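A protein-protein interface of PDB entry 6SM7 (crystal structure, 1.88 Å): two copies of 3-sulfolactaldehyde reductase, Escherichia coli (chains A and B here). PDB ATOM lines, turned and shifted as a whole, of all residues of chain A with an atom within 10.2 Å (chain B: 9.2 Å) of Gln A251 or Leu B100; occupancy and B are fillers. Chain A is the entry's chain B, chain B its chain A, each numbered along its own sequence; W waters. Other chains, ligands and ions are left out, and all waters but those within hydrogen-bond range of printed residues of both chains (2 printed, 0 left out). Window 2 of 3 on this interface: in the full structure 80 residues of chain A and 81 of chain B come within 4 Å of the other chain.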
ATOM      1  N   LEU A 191      27.484 -16.434 -22.243  1.00  0.00           N
ATOM      2  CA  LEU A 191      27.599 -15.456 -21.132  1.00  0.00           C
ATOM      3  C   LEU A 191      29.070 -15.398 -20.672  1.00  0.00           C
ATOM      4  O   LEU A 191      29.596 -14.299 -20.409  1.00  0.00           O
ATOM      5  CB  LEU A 191      26.670 -15.881 -19.995  1.00  0.00           C
ATOM      6  CG  LEU A 191      26.581 -14.851 -18.871  1.00  0.00           C
ATOM      7  CD1 LEU A 191      26.086 -13.544 -19.420  1.00  0.00           C
ATOM      8  CD2 LEU A 191      25.669 -15.358 -17.758  1.00  0.00           C
ATOM      9  N   CYS A 192      29.701 -16.558 -20.573  1.00  0.00           N
ATOM     10  CA  CYS A 192      31.116 -16.708 -20.178  1.00  0.00           C
ATOM     11  C   CYS A 192      32.006 -15.862 -21.096  1.00  0.00           C
ATOM     12  O   CYS A 192      32.819 -15.046 -20.627  1.00  0.00           O
ATOM     13  CB  CYS A 192      31.455 -18.186 -20.204  1.00  0.00           C
ATOM     14  SG  CYS A 192      33.079 -18.495 -19.452  1.00  0.00           S
ATOM     15  N   ALA A 194      31.058 -13.397 -23.097  1.00  0.00           N
ATOM     16  CA  ALA A 194      30.699 -11.961 -23.020  1.00  0.00           C
ATOM     17  C   ALA A 194      31.340 -11.329 -21.786  1.00  0.00           C
ATOM     18  O   ALA A 194      31.566 -10.133 -21.827  1.00  0.00           O
ATOM     19  CB  ALA A 194      29.210 -11.770 -23.001  1.00  0.00           C
ATOM     20  N   LEU A 195      31.582 -12.103 -20.732  1.00  0.00           N
ATOM     21  CA  LEU A 195      32.228 -11.600 -19.482  1.00  0.00           C
ATOM     22  C   LEU A 195      33.756 -11.645 -19.622  1.00  0.00           C
ATOM     23  O   LEU A 195      34.447 -11.273 -18.662  1.00  0.00           O
ATOM     24  CB  LEU A 195      31.772 -12.493 -18.329  1.00  0.00           C
ATOM     25  CG  LEU A 195      30.395 -12.169 -17.760  1.00  0.00           C
ATOM     26  CD1 LEU A 195      29.931 -13.265 -16.844  1.00  0.00           C
ATOM     27  CD2 LEU A 195      30.453 -10.841 -17.036  1.00  0.00           C
ATOM     28  N   ASN A 196      34.279 -12.101 -20.767  1.00  0.00           N
ATOM     29  CA  ASN A 196      35.740 -12.207 -21.023  1.00  0.00           C
ATOM     30  C   ASN A 196      36.379 -13.227 -20.080  1.00  0.00           C
ATOM     31  O   ASN A 196      37.530 -13.040 -19.705  1.00  0.00           O
ATOM     32  CB  ASN A 196      36.398 -10.828 -20.918  1.00  0.00           C
ATOM     33  CG  ASN A 196      35.959  -9.939 -22.054  1.00  0.00           C
ATOM     34  OD1 ASN A 196      36.123 -10.335 -23.210  1.00  0.00           O
ATOM     35  ND2 ASN A 196      35.371  -8.785 -21.743  1.00  0.00           N
ATOM     36  N   LEU A 197      35.657 -14.281 -19.692  1.00  0.00           N
ATOM     37  CA  LEU A 197      36.231 -15.383 -18.886  1.00  0.00           C
ATOM     38  C   LEU A 197      36.589 -16.503 -19.849  1.00  0.00           C
ATOM     39  O   LEU A 197      35.707 -16.988 -20.554  1.00  0.00           O
ATOM     40  CB  LEU A 197      35.238 -15.838 -17.832  1.00  0.00           C
ATOM     41  CG  LEU A 197      35.671 -17.044 -16.999  1.00  0.00           C
ATOM     42  CD1 LEU A 197      36.830 -16.718 -16.072  1.00  0.00           C
ATOM     43  CD2 LEU A 197      34.526 -17.560 -16.172  1.00  0.00           C
ATOM     44  N   GLY A 243      18.804 -14.262 -10.842  1.00  0.00           N
ATOM     45  CA  GLY A 243      18.495 -12.856 -11.140  1.00  0.00           C
ATOM     46  C   GLY A 243      19.768 -12.115 -11.486  1.00  0.00           C
ATOM     47  O   GLY A 243      19.749 -11.314 -12.426  1.00  0.00           O
ATOM     48  N   ILE A 244      20.876 -12.377 -10.761  1.00  0.00           N
ATOM     49  CA  ILE A 244      22.189 -11.733 -11.091  1.00  0.00           C
ATOM     50  C   ILE A 244      22.642 -12.163 -12.497  1.00  0.00           C
ATOM     51  O   ILE A 244      23.035 -11.304 -13.278  1.00  0.00           O
ATOM     52  CB  ILE A 244      23.267 -12.053 -10.036  1.00  0.00           C
ATOM     53  CG1 ILE A 244      22.906 -11.440  -8.673  1.00  0.00           C
ATOM     54  CG2 ILE A 244      24.640 -11.598 -10.518  1.00  0.00           C
ATOM     55  CD1 ILE A 244      22.677  -9.924  -8.729  1.00  0.00           C
ATOM     56  N   ALA A 245      22.615 -13.444 -12.792  1.00  0.00           N
ATOM     57  CA  ALA A 245      23.007 -13.949 -14.131  1.00  0.00           C
ATOM     58  C   ALA A 245      22.173 -13.265 -15.214  1.00  0.00           C
ATOM     59  O   ALA A 245      22.742 -12.874 -16.239  1.00  0.00           O
ATOM     60  CB  ALA A 245      22.833 -15.449 -14.170  1.00  0.00           C
ATOM     61  N   LEU A 246      20.849 -13.156 -15.028  1.00  0.00           N
ATOM     62  CA  LEU A 246      19.960 -12.526 -16.029  1.00  0.00           C
ATOM     63  C   LEU A 246      20.219 -11.022 -16.119  1.00  0.00           C
ATOM     64  O   LEU A 246      20.125 -10.459 -17.223  1.00  0.00           O
ATOM     65  CB  LEU A 246      18.516 -12.873 -15.683  1.00  0.00           C
ATOM     66  CG  LEU A 246      18.155 -14.302 -16.078  1.00  0.00           C
ATOM     67  CD1 LEU A 246      16.898 -14.757 -15.357  1.00  0.00           C
ATOM     68  CD2 LEU A 246      18.018 -14.406 -17.596  1.00  0.00           C
ATOM     69  N   ASP A 247      20.575 -10.382 -15.006  1.00  0.00           N
ATOM     70  CA  ASP A 247      20.923  -8.937 -15.004  1.00  0.00           C
ATOM     71  C   ASP A 247      22.142  -8.738 -15.897  1.00  0.00           C
ATOM     72  O   ASP A 247      22.137  -7.827 -16.732  1.00  0.00           O
ATOM     73  CB  ASP A 247      21.271  -8.426 -13.594  1.00  0.00           C
ATOM     74  CG  ASP A 247      20.079  -8.262 -12.652  1.00  0.00           C
ATOM     75  OD1 ASP A 247      18.933  -8.104 -13.155  1.00  0.00           O
ATOM     76  OD2 ASP A 247      20.299  -8.300 -11.385  1.00  0.00           O
ATOM     77  N   VAL A 248      23.165  -9.564 -15.692  1.00  0.00           N
ATOM     78  CA  VAL A 248      24.444  -9.485 -16.450  1.00  0.00           C
ATOM     79  C   VAL A 248      24.164  -9.799 -17.922  1.00  0.00           C
ATOM     80  O   VAL A 248      24.613  -9.049 -18.771  1.00  0.00           O
ATOM     81  CB  VAL A 248      25.475 -10.463 -15.870  1.00  0.00           C
ATOM     82  CG1 VAL A 248      26.706 -10.588 -16.761  1.00  0.00           C
ATOM     83  CG2 VAL A 248      25.872 -10.069 -14.459  1.00  0.00           C
ATOM     84  N   ALA A 249      23.413 -10.869 -18.204  1.00  0.00           N
ATOM     85  CA  ALA A 249      23.108 -11.290 -19.586  1.00  0.00           C
ATOM     86  C   ALA A 249      22.403 -10.141 -20.298  1.00  0.00           C
ATOM     87  O   ALA A 249      22.756  -9.825 -21.470  1.00  0.00           O
ATOM     88  CB  ALA A 249      22.280 -12.541 -19.589  1.00  0.00           C
ATOM     89  N   ASN A 250      21.449  -9.503 -19.629  1.00  0.00           N
ATOM     90  CA  ASN A 250      20.663  -8.406 -20.241  1.00  0.00           C
ATOM     91  C   ASN A 250      21.546  -7.171 -20.439  1.00  0.00           C
ATOM     92  O   ASN A 250      21.351  -6.475 -21.418  1.00  0.00           O
ATOM     93  CB  ASN A 250      19.353  -8.188 -19.501  1.00  0.00           C
ATOM     94  CG  ASN A 250      18.292  -9.139 -20.012  1.00  0.00           C
ATOM     95  OD1 ASN A 250      17.698  -8.842 -21.041  1.00  0.00           O
ATOM     96  ND2 ASN A 250      18.141 -10.304 -19.393  1.00  0.00           N
ATOM     97  N   GLN A 251      22.505  -6.908 -19.553  1.00  0.00           N
ATOM     98  CA  GLN A 251      23.430  -5.769 -19.744  1.00  0.00           C
ATOM     99  C   GLN A 251      24.381  -6.063 -20.912  1.00  0.00           C
ATOM    100  O   GLN A 251      24.744  -5.116 -21.606  1.00  0.00           O
ATOM    101  CB  GLN A 251      24.225  -5.512 -18.474  1.00  0.00           C
ATOM    102  CG  GLN A 251      23.484  -4.760 -17.402  1.00  0.00           C
ATOM    103  CD  GLN A 251      24.505  -4.456 -16.328  1.00  0.00           C
ATOM    104  OE1 GLN A 251      24.601  -5.159 -15.332  1.00  0.00           O
ATOM    105  NE2 GLN A 251      25.385  -3.510 -16.617  1.00  0.00           N
ATOM    106  N   LEU A 252      24.774  -7.314 -21.111  1.00  0.00           N
ATOM    107  CA  LEU A 252      25.740  -7.724 -22.166  1.00  0.00           C
ATOM    108  C   LEU A 252      25.022  -8.196 -23.440  1.00  0.00           C
ATOM    109  O   LEU A 252      25.716  -8.644 -24.369  1.00  0.00           O
ATOM    110  CB  LEU A 252      26.646  -8.817 -21.586  1.00  0.00           C
ATOM    111  CG  LEU A 252      27.512  -8.385 -20.394  1.00  0.00           C
ATOM    112  CD1 LEU A 252      28.383  -9.524 -19.937  1.00  0.00           C
ATOM    113  CD2 LEU A 252      28.365  -7.173 -20.730  1.00  0.00           C
ATOM    114  N   HIS A 253      23.695  -8.063 -23.530  1.00  0.00           N
ATOM    115  CA  HIS A 253      22.837  -8.554 -24.639  1.00  0.00           C
ATOM    116  C   HIS A 253      23.218  -9.982 -25.061  1.00  0.00           C
ATOM    117  O   HIS A 253      23.382 -10.286 -26.289  1.00  0.00           O
ATOM    118  CB  HIS A 253      22.779  -7.532 -25.780  1.00  0.00           C
ATOM    119  CG  HIS A 253      24.070  -7.165 -26.418  1.00  0.00           C
ATOM    120  ND1 HIS A 253      24.824  -8.075 -27.153  1.00  0.00           N
ATOM    121  CD2 HIS A 253      24.691  -5.975 -26.502  1.00  0.00           C
ATOM    122  CE1 HIS A 253      25.920  -7.470 -27.603  1.00  0.00           C
ATOM    123  NE2 HIS A 253      25.843  -6.163 -27.249  1.00  0.00           N
ATOM    124  N   VAL A 254      23.312 -10.871 -24.085  1.00  0.00           N
ATOM    125  CA  VAL A 254      23.349 -12.326 -24.307  1.00  0.00           C
ATOM    126  C   VAL A 254      21.943 -12.855 -24.032  1.00  0.00           C
ATOM    127  O   VAL A 254      21.533 -12.948 -22.861  1.00  0.00           O
ATOM    128  CB  VAL A 254      24.395 -13.002 -23.410  1.00  0.00           C
ATOM    129  CG1 VAL A 254      24.372 -14.510 -23.618  1.00  0.00           C
ATOM    130  CG2 VAL A 254      25.786 -12.452 -23.635  1.00  0.00           C
ATOM    131  N   PRO A 255      21.157 -13.210 -25.067  1.00  0.00           N
ATOM    132  CA  PRO A 255      19.812 -13.733 -24.852  1.00  0.00           C
ATOM    133  C   PRO A 255      19.886 -15.090 -24.156  1.00  0.00           C
ATOM    134  O   PRO A 255      20.625 -15.972 -24.569  1.00  0.00           O
ATOM    135  CB  PRO A 255      19.170 -13.851 -26.244  1.00  0.00           C
ATOM    136  CG  PRO A 255      20.039 -12.925 -27.104  1.00  0.00           C
ATOM    137  CD  PRO A 255      21.426 -13.039 -26.509  1.00  0.00           C
ATOM    138  N   MET A 256      19.155 -15.201 -23.056  1.00  0.00           N
ATOM    139  CA  MET A 256      19.134 -16.433 -22.242  1.00  0.00           C
ATOM    140  C   MET A 256      17.689 -16.853 -21.988  1.00  0.00           C
ATOM    141  O   MET A 256      17.204 -16.785 -20.849  1.00  0.00           O
ATOM    142  CB  MET A 256      19.894 -16.236 -20.929  1.00  0.00           C
ATOM    143  CG  MET A 256      21.362 -15.893 -21.174  1.00  0.00           C
ATOM    144  SD  MET A 256      22.523 -16.386 -19.887  1.00  0.00           S
ATOM    145  CE  MET A 256      21.649 -15.824 -18.422  1.00  0.00           C
ATOM    146  N   GLY B  68      25.858  -6.979  -3.688  1.00  0.00           N
ATOM    147  CA  GLY B  68      26.857  -5.956  -4.031  1.00  0.00           C
ATOM    148  C   GLY B  68      26.546  -4.599  -3.407  1.00  0.00           C
ATOM    149  O   GLY B  68      27.506  -3.869  -3.146  1.00  0.00           O
ATOM    150  N   ARG B  72      29.330  -2.690  -1.123  1.00  0.00           N
ATOM    151  CA  ARG B  72      29.724  -1.272  -1.366  1.00  0.00           C
ATOM    152  C   ARG B  72      29.526  -0.462  -0.072  1.00  0.00           C
ATOM    153  O   ARG B  72      30.415   0.319   0.265  1.00  0.00           O
ATOM    154  CB  ARG B  72      28.939  -0.670  -2.528  1.00  0.00           C
ATOM    155  CG  ARG B  72      29.178   0.826  -2.722  1.00  0.00           C
ATOM    156  CD  ARG B  72      28.698   1.284  -4.093  1.00  0.00           C
ATOM    157  NE  ARG B  72      29.550   0.754  -5.144  1.00  0.00           N
ATOM    158  CZ  ARG B  72      30.731   1.253  -5.484  1.00  0.00           C
ATOM    159  NH1 ARG B  72      31.219   2.293  -4.849  1.00  0.00           N
ATOM    160  NH2 ARG B  72      31.445   0.700  -6.439  1.00  0.00           N
ATOM    161  N   ILE B  97      28.248 -11.739  -5.770  1.00  0.00           N
ATOM    162  CA  ILE B  97      27.561 -10.484  -6.159  1.00  0.00           C
ATOM    163  C   ILE B  97      27.666 -10.313  -7.674  1.00  0.00           C
ATOM    164  O   ILE B  97      28.296 -11.160  -8.341  1.00  0.00           O
ATOM    165  CB  ILE B  97      28.165  -9.296  -5.393  1.00  0.00           C
ATOM    166  CG1 ILE B  97      29.609  -9.007  -5.801  1.00  0.00           C
ATOM    167  CG2 ILE B  97      28.009  -9.529  -3.916  1.00  0.00           C
ATOM    168  CD1 ILE B  97      30.145  -7.686  -5.312  1.00  0.00           C
ATOM    169  N   HIS B  98      27.091  -9.240  -8.194  1.00  0.00           N
ATOM    170  CA  HIS B  98      27.128  -8.934  -9.635  1.00  0.00           C
ATOM    171  C   HIS B  98      28.584  -8.692 -10.029  1.00  0.00           C
ATOM    172  O   HIS B  98      29.287  -7.880  -9.411  1.00  0.00           O
ATOM    173  CB  HIS B  98      26.170  -7.774  -9.872  1.00  0.00           C
ATOM    174  CG  HIS B  98      25.885  -7.454 -11.284  1.00  0.00           C
ATOM    175  ND1 HIS B  98      26.886  -7.225 -12.221  1.00  0.00           N
ATOM    176  CD2 HIS B  98      24.692  -7.257 -11.894  1.00  0.00           C
ATOM    177  CE1 HIS B  98      26.321  -6.897 -13.366  1.00  0.00           C
ATOM    178  NE2 HIS B  98      24.976  -6.891 -13.186  1.00  0.00           N
ATOM    179  N   PRO B  99      29.093  -9.365 -11.085  1.00  0.00           N
ATOM    180  CA  PRO B  99      30.492  -9.220 -11.468  1.00  0.00           C
ATOM    181  C   PRO B  99      30.873  -7.812 -11.913  1.00  0.00           C
ATOM    182  O   PRO B  99      32.017  -7.402 -11.698  1.00  0.00           O
ATOM    183  CB  PRO B  99      30.743 -10.220 -12.626  1.00  0.00           C
ATOM    184  CG  PRO B  99      29.414 -10.853 -12.887  1.00  0.00           C
ATOM    185  CD  PRO B  99      28.382 -10.363 -11.892  1.00  0.00           C
ATOM    186  N   LEU B 100      29.938  -7.061 -12.511  1.00  0.00           N
ATOM    187  CA  LEU B 100      30.261  -5.679 -12.938  1.00  0.00           C
ATOM    188  C   LEU B 100      30.329  -4.787 -11.690  1.00  0.00           C
ATOM    189  O   LEU B 100      31.111  -3.804 -11.684  1.00  0.00           O
ATOM    190  CB  LEU B 100      29.284  -5.237 -14.043  1.00  0.00           C
ATOM    191  CG  LEU B 100      29.184  -6.232 -15.225  1.00  0.00           C
ATOM    192  CD1 LEU B 100      28.268  -5.739 -16.342  1.00  0.00           C
ATOM    193  CD2 LEU B 100      30.559  -6.579 -15.787  1.00  0.00           C
ATOM    194  N   GLN B 101      29.635  -5.149 -10.611  1.00  0.00           N
ATOM    195  CA  GLN B 101      29.769  -4.428  -9.313  1.00  0.00           C
ATOM    196  C   GLN B 101      31.144  -4.751  -8.718  1.00  0.00           C
ATOM    197  O   GLN B 101      31.791  -3.840  -8.212  1.00  0.00           O
ATOM    198  CB  GLN B 101      28.675  -4.805  -8.315  1.00  0.00           C
ATOM    199  CG  GLN B 101      27.277  -4.271  -8.619  1.00  0.00           C
ATOM    200  CD  GLN B 101      26.307  -4.807  -7.577  1.00  0.00           C
ATOM    201  OE1 GLN B 101      26.260  -6.001  -7.290  1.00  0.00           O
ATOM    202  NE2 GLN B 101      25.497  -3.947  -7.014  1.00  0.00           N
ATOM    203  N   THR B 102      31.584  -6.005  -8.763  1.00  0.00           N
ATOM    204  CA  THR B 102      32.944  -6.394  -8.330  1.00  0.00           C
ATOM    205  C   THR B 102      33.976  -5.527  -9.063  1.00  0.00           C
ATOM    206  O   THR B 102      34.853  -4.969  -8.406  1.00  0.00           O
ATOM    207  CB  THR B 102      33.211  -7.883  -8.562  1.00  0.00           C
ATOM    208  OG1 THR B 102      32.289  -8.666  -7.793  1.00  0.00           O
ATOM    209  CG2 THR B 102      34.627  -8.239  -8.201  1.00  0.00           C
ATOM    210  N   ASP B 103      33.889  -5.427 -10.387  1.00  0.00           N
ATOM    211  CA  ASP B 103      34.858  -4.635 -11.190  1.00  0.00           C
ATOM    212  C   ASP B 103      34.888  -3.194 -10.655  1.00  0.00           C
ATOM    213  O   ASP B 103      35.993  -2.636 -10.465  1.00  0.00           O
ATOM    214  CB  ASP B 103      34.542  -4.617 -12.689  1.00  0.00           C
ATOM    215  CG  ASP B 103      34.585  -5.975 -13.367  1.00  0.00           C
ATOM    216  OD1 ASP B 103      35.196  -6.924 -12.807  1.00  0.00           O
ATOM    217  OD2 ASP B 103      33.970  -6.070 -14.458  1.00  0.00           O
ATOM    218  N   LYS B 104      33.721  -2.609 -10.423  1.00  0.00           N
ATOM    219  CA  LYS B 104      33.622  -1.194 -10.007  1.00  0.00           C
ATOM    220  C   LYS B 104      34.186  -1.024  -8.583  1.00  0.00           C
ATOM    221  O   LYS B 104      34.881  -0.003  -8.333  1.00  0.00           O
ATOM    222  CB  LYS B 104      32.200  -0.666 -10.160  1.00  0.00           C
ATOM    223  CG  LYS B 104      32.110   0.857 -10.208  1.00  0.00           C
ATOM    224  N   LEU B 105      33.929  -1.968  -7.677  1.00  0.00           N
ATOM    225  CA  LEU B 105      34.500  -1.927  -6.302  1.00  0.00           C
ATOM    226  C   LEU B 105      36.017  -2.007  -6.372  1.00  0.00           C
ATOM    227  O   LEU B 105      36.701  -1.209  -5.684  1.00  0.00           O
ATOM    228  CB  LEU B 105      33.926  -3.060  -5.454  1.00  0.00           C
ATOM    229  CG  LEU B 105      32.444  -2.935  -5.114  1.00  0.00           C
ATOM    230  CD1 LEU B 105      31.911  -4.260  -4.605  1.00  0.00           C
ATOM    231  CD2 LEU B 105      32.204  -1.815  -4.113  1.00  0.00           C
ATOM    232  N   ILE B 106      36.551  -2.923  -7.178  1.00  0.00           N
ATOM    233  CA  ILE B 106      38.022  -3.087  -7.296  1.00  0.00           C
ATOM    234  C   ILE B 106      38.622  -1.770  -7.828  1.00  0.00           C
ATOM    235  O   ILE B 106      39.639  -1.308  -7.266  1.00  0.00           O
ATOM    236  CB  ILE B 106      38.392  -4.309  -8.151  1.00  0.00           C
ATOM    237  CG1 ILE B 106      38.020  -5.612  -7.437  1.00  0.00           C
ATOM    238  CG2 ILE B 106      39.861  -4.260  -8.530  1.00  0.00           C
ATOM    239  CD1 ILE B 106      38.199  -6.856  -8.297  1.00  0.00           C
ATOM    240  N   ALA B 107      38.031  -1.191  -8.871  1.00  0.00           N
ATOM    241  CA  ALA B 107      38.495   0.077  -9.488  1.00  0.00           C
ATOM    242  C   ALA B 107      38.427   1.228  -8.466  1.00  0.00           C
ATOM    243  O   ALA B 107      39.413   1.998  -8.365  1.00  0.00           O
ATOM    244  CB  ALA B 107      37.683   0.393 -10.732  1.00  0.00           C
ATOM    245  N   ASP B 108      37.326   1.334  -7.728  1.00  0.00           N
ATOM    246  CA  ASP B 108      37.102   2.433  -6.750  1.00  0.00           C
ATOM    247  C   ASP B 108      38.122   2.302  -5.614  1.00  0.00           C
ATOM    248  O   ASP B 108      38.633   3.349  -5.148  1.00  0.00           O
ATOM    249  CB  ASP B 108      35.662   2.463  -6.239  1.00  0.00           C
ATOM    250  CG  ASP B 108      34.633   2.889  -7.278  1.00  0.00           C
ATOM    251  OD1 ASP B 108      35.033   3.432  -8.271  1.00  0.00           O
ATOM    252  OD2 ASP B 108      33.423   2.668  -7.073  1.00  0.00           O
ATOM    253  N   ASP B 118      38.635 -10.585  -5.719  1.00  0.00           N
ATOM    254  CA  ASP B 118      37.372 -11.350  -5.627  1.00  0.00           C
ATOM    255  C   ASP B 118      37.722 -12.823  -5.434  1.00  0.00           C
ATOM    256  O   ASP B 118      38.315 -13.413  -6.342  1.00  0.00           O
ATOM    257  CB  ASP B 118      36.506 -11.155  -6.874  1.00  0.00           C
ATOM    258  CG  ASP B 118      37.261 -11.389  -8.182  1.00  0.00           C
ATOM    259  OD1 ASP B 118      38.401 -10.846  -8.310  1.00  0.00           O
ATOM    260  OD2 ASP B 118      36.732 -12.129  -9.062  1.00  0.00           O
ATOM    261  N   GLY B 165      38.419 -10.041 -11.004  1.00  0.00           N
ATOM    262  CA  GLY B 165      37.028 -10.141 -11.474  1.00  0.00           C
ATOM    263  C   GLY B 165      36.741 -11.487 -12.105  1.00  0.00           C
ATOM    264  O   GLY B 165      35.552 -11.759 -12.369  1.00  0.00           O
ATOM    265  N   ILE B 168      34.627 -13.998  -9.456  1.00  0.00           N
ATOM    266  CA  ILE B 168      33.164 -13.789  -9.398  1.00  0.00           C
ATOM    267  C   ILE B 168      32.570 -14.226 -10.752  1.00  0.00           C
ATOM    268  O   ILE B 168      31.484 -14.785 -10.746  1.00  0.00           O
ATOM    269  CB  ILE B 168      32.795 -12.344  -9.019  1.00  0.00           C
ATOM    270  CG1 ILE B 168      31.291 -12.238  -8.838  1.00  0.00           C
ATOM    271  CG2 ILE B 168      33.312 -11.330 -10.012  1.00  0.00           C
ATOM    272  CD1 ILE B 168      30.674 -13.286  -7.937  1.00  0.00           C
ATOM    273  N   ARG B 169      33.261 -14.010 -11.864  1.00  0.00           N
ATOM    274  CA  ARG B 169      32.747 -14.431 -13.200  1.00  0.00           C
ATOM    275  C   ARG B 169      32.569 -15.942 -13.229  1.00  0.00           C
ATOM    276  O   ARG B 169      31.463 -16.400 -13.647  1.00  0.00           O
ATOM    277  CB  ARG B 169      33.634 -13.922 -14.332  1.00  0.00           C
ATOM    278  CG  ARG B 169      33.449 -12.448 -14.629  1.00  0.00           C
ATOM    279  CD  ARG B 169      34.609 -11.929 -15.470  1.00  0.00           C
ATOM    280  NE  ARG B 169      34.363 -10.610 -16.034  1.00  0.00           N
ATOM    281  CZ  ARG B 169      34.295  -9.483 -15.332  1.00  0.00           C
ATOM    282  NH1 ARG B 169      34.464  -9.489 -14.015  1.00  0.00           N
ATOM    283  NH2 ARG B 169      34.032  -8.348 -15.951  1.00  0.00           N
ATOM    284  N   LEU B 172      29.732 -17.083 -11.079  1.00  0.00           N
ATOM    285  CA  LEU B 172      28.427 -16.754 -11.680  1.00  0.00           C
ATOM    286  C   LEU B 172      28.108 -17.724 -12.820  1.00  0.00           C
ATOM    287  O   LEU B 172      26.970 -18.172 -12.910  1.00  0.00           O
ATOM    288  CB  LEU B 172      28.408 -15.310 -12.150  1.00  0.00           C
ATOM    289  CG  LEU B 172      27.062 -14.918 -12.754  1.00  0.00           C
ATOM    290  CD1 LEU B 172      25.971 -15.034 -11.698  1.00  0.00           C
ATOM    291  CD2 LEU B 172      27.099 -13.552 -13.389  1.00  0.00           C
ATOM    292  N   ALA B 290      23.723 -13.181 -29.708  1.00  0.00           N
ATOM    293  CA  ALA B 290      24.350 -12.272 -28.722  1.00  0.00           C
ATOM    294  C   ALA B 290      25.186 -11.191 -29.399  1.00  0.00           C
ATOM    295  O   ALA B 290      25.761 -10.383 -28.676  1.00  0.00           O
ATOM    296  CB  ALA B 290      25.159 -13.063 -27.742  1.00  0.00           C
HETATM  297  O   HOH W   1      34.578  -7.818 -18.860  1.00  0.00           O
HETATM  298  O   HOH W   2      27.090 -10.297 -26.162  1.00  0.00           O
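The backbone carbonyl oxygen (O) of Leu A195 sits at hydrogen-bond distance from the guanidinium group (NE) of Arg B169, at 2.7 Å. ND1 of His A253 is in hydrogen-bond range of O of Ala B290, 2.9 Å away. The side-chain amide oxygen (OE1) of Gln A251 lies within hydrogen-bond range of a ring nitrogen (NE2) of His B98.
The backbone carbonyl oxygen (O) of Ala A249 sits at hydrogen-bond distance from the backbone NH (N) of Val A254 (2.9 Å). The guanidinium group of Arg B169 lies within salt-bridge range of the side-chain carboxylate of Asp B103, at 2.7 Å. The side-chain amide oxygen (OE1) of Gln B101 sits close to the backbone NH (N) of His B98, at 3.5 Å. A ring nitrogen (ND1) of His B98 sits at hydrogen-bond distance from the backbone NH (N) of Leu B100 (3.1 Å). O of Gly B165 lies within hydrogen-bond range of NH1 of Arg B169 (3.0 Å). The backbone carbonyl oxygen (O) of His B98 sits at hydrogen-bond distance from the side-chain hydroxyl (OG1) of Thr B102 (3.5 Å).
Leu A197 touches Arg B169. His B98 touches Ile A244 (CA to CG2, 3.8 Å). CG2 of Ile A244 touches CD1 of Leu B172, 3.9 Å away. CD1 of Leu B172 touches N of Ala A245 (3.9 Å). His B98 touches Asp A247. Val A248 touches His B98 (CG2 to CE1, 3.4 Å). Val A248 touches Pro B99 (CG2 to CD, 3.6 Å). Val A248 touches Leu B172 (CG2 to CD2, 3.8 Å). NE2 of Gln A251 touches CD1 of Leu B100, at 3.7 Å. CA of Val A254 touches CB of Ala B290 (3.95 Å).
Of the printed residues of chain A, Leu B100 touches Gln A251. Of chain A, only Val A248 (3.6 Å) comes within 4 Å of Pro B99. No residue of chain A comes within 4 Å of Asp B103. Of the printed residues of chain A, Leu B172 touches Ile A244, Ala A245 and Val A248. Printed residues of chain B within 4 Å of Ile A244: His B98 (3.8 Å) and Leu B172 (3.9 Å). Of the printed residues of chain B, Leu A197 touches Arg B169 (3.9 Å). Gly B68 touches none of the printed residues of chain A. Asp B108 touches none of the printed residues of chain A. The nearest residue of chain B that does not touch Gln A251 is Gln B101 (6.9 Å). The nearest residue of chain A that does not touch Leu B100 is Leu A195 (4.4 Å). The nearest printed residue of chain B that does not touch Val A248 is Leu B100 (5.1 Å).
Hydrophobic or aromatic side chains of chain A that line the printed part of chain B: Leu A195, Leu A197, Ile A244, Val A248, His A253 and Pro A255. Along chain A the printed residues that touch a printed residue of chain B span positions 195 to 255. Of the 20 printed residues of chain B, 6 touch a printed residue of chain A. Hydrophobic or aromatic side chains of chain B that line the printed part of chain A: His B98, Pro B99, Leu B100, Leu B172 and Ala B290. Among the printed residues, no Asp or Glu carboxylate lies within 4 Å of a Lys or Arg side-chain nitrogen of the other chain.
No position is printed for both chains. Of the 14 pairs that touch across the chains among the printed residues, none has its exchanged pair printed and touching as well.
Water W2 lies within hydrogen-bond range of the backbone carbonyl oxygen of Leu A252 (2.8 Å), the backbone carbonyl oxygen of Ala B290 (2.8 Å) and a ring nitrogen (ND1) of His A253 (3.3 Å). Water W1 lies within hydrogen-bond range of the guanidinium group (NH2) of Arg B169, the side-chain amide nitrogen (ND2) of Asn A196 and the backbone carbonyl oxygen (O) of Leu A195.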
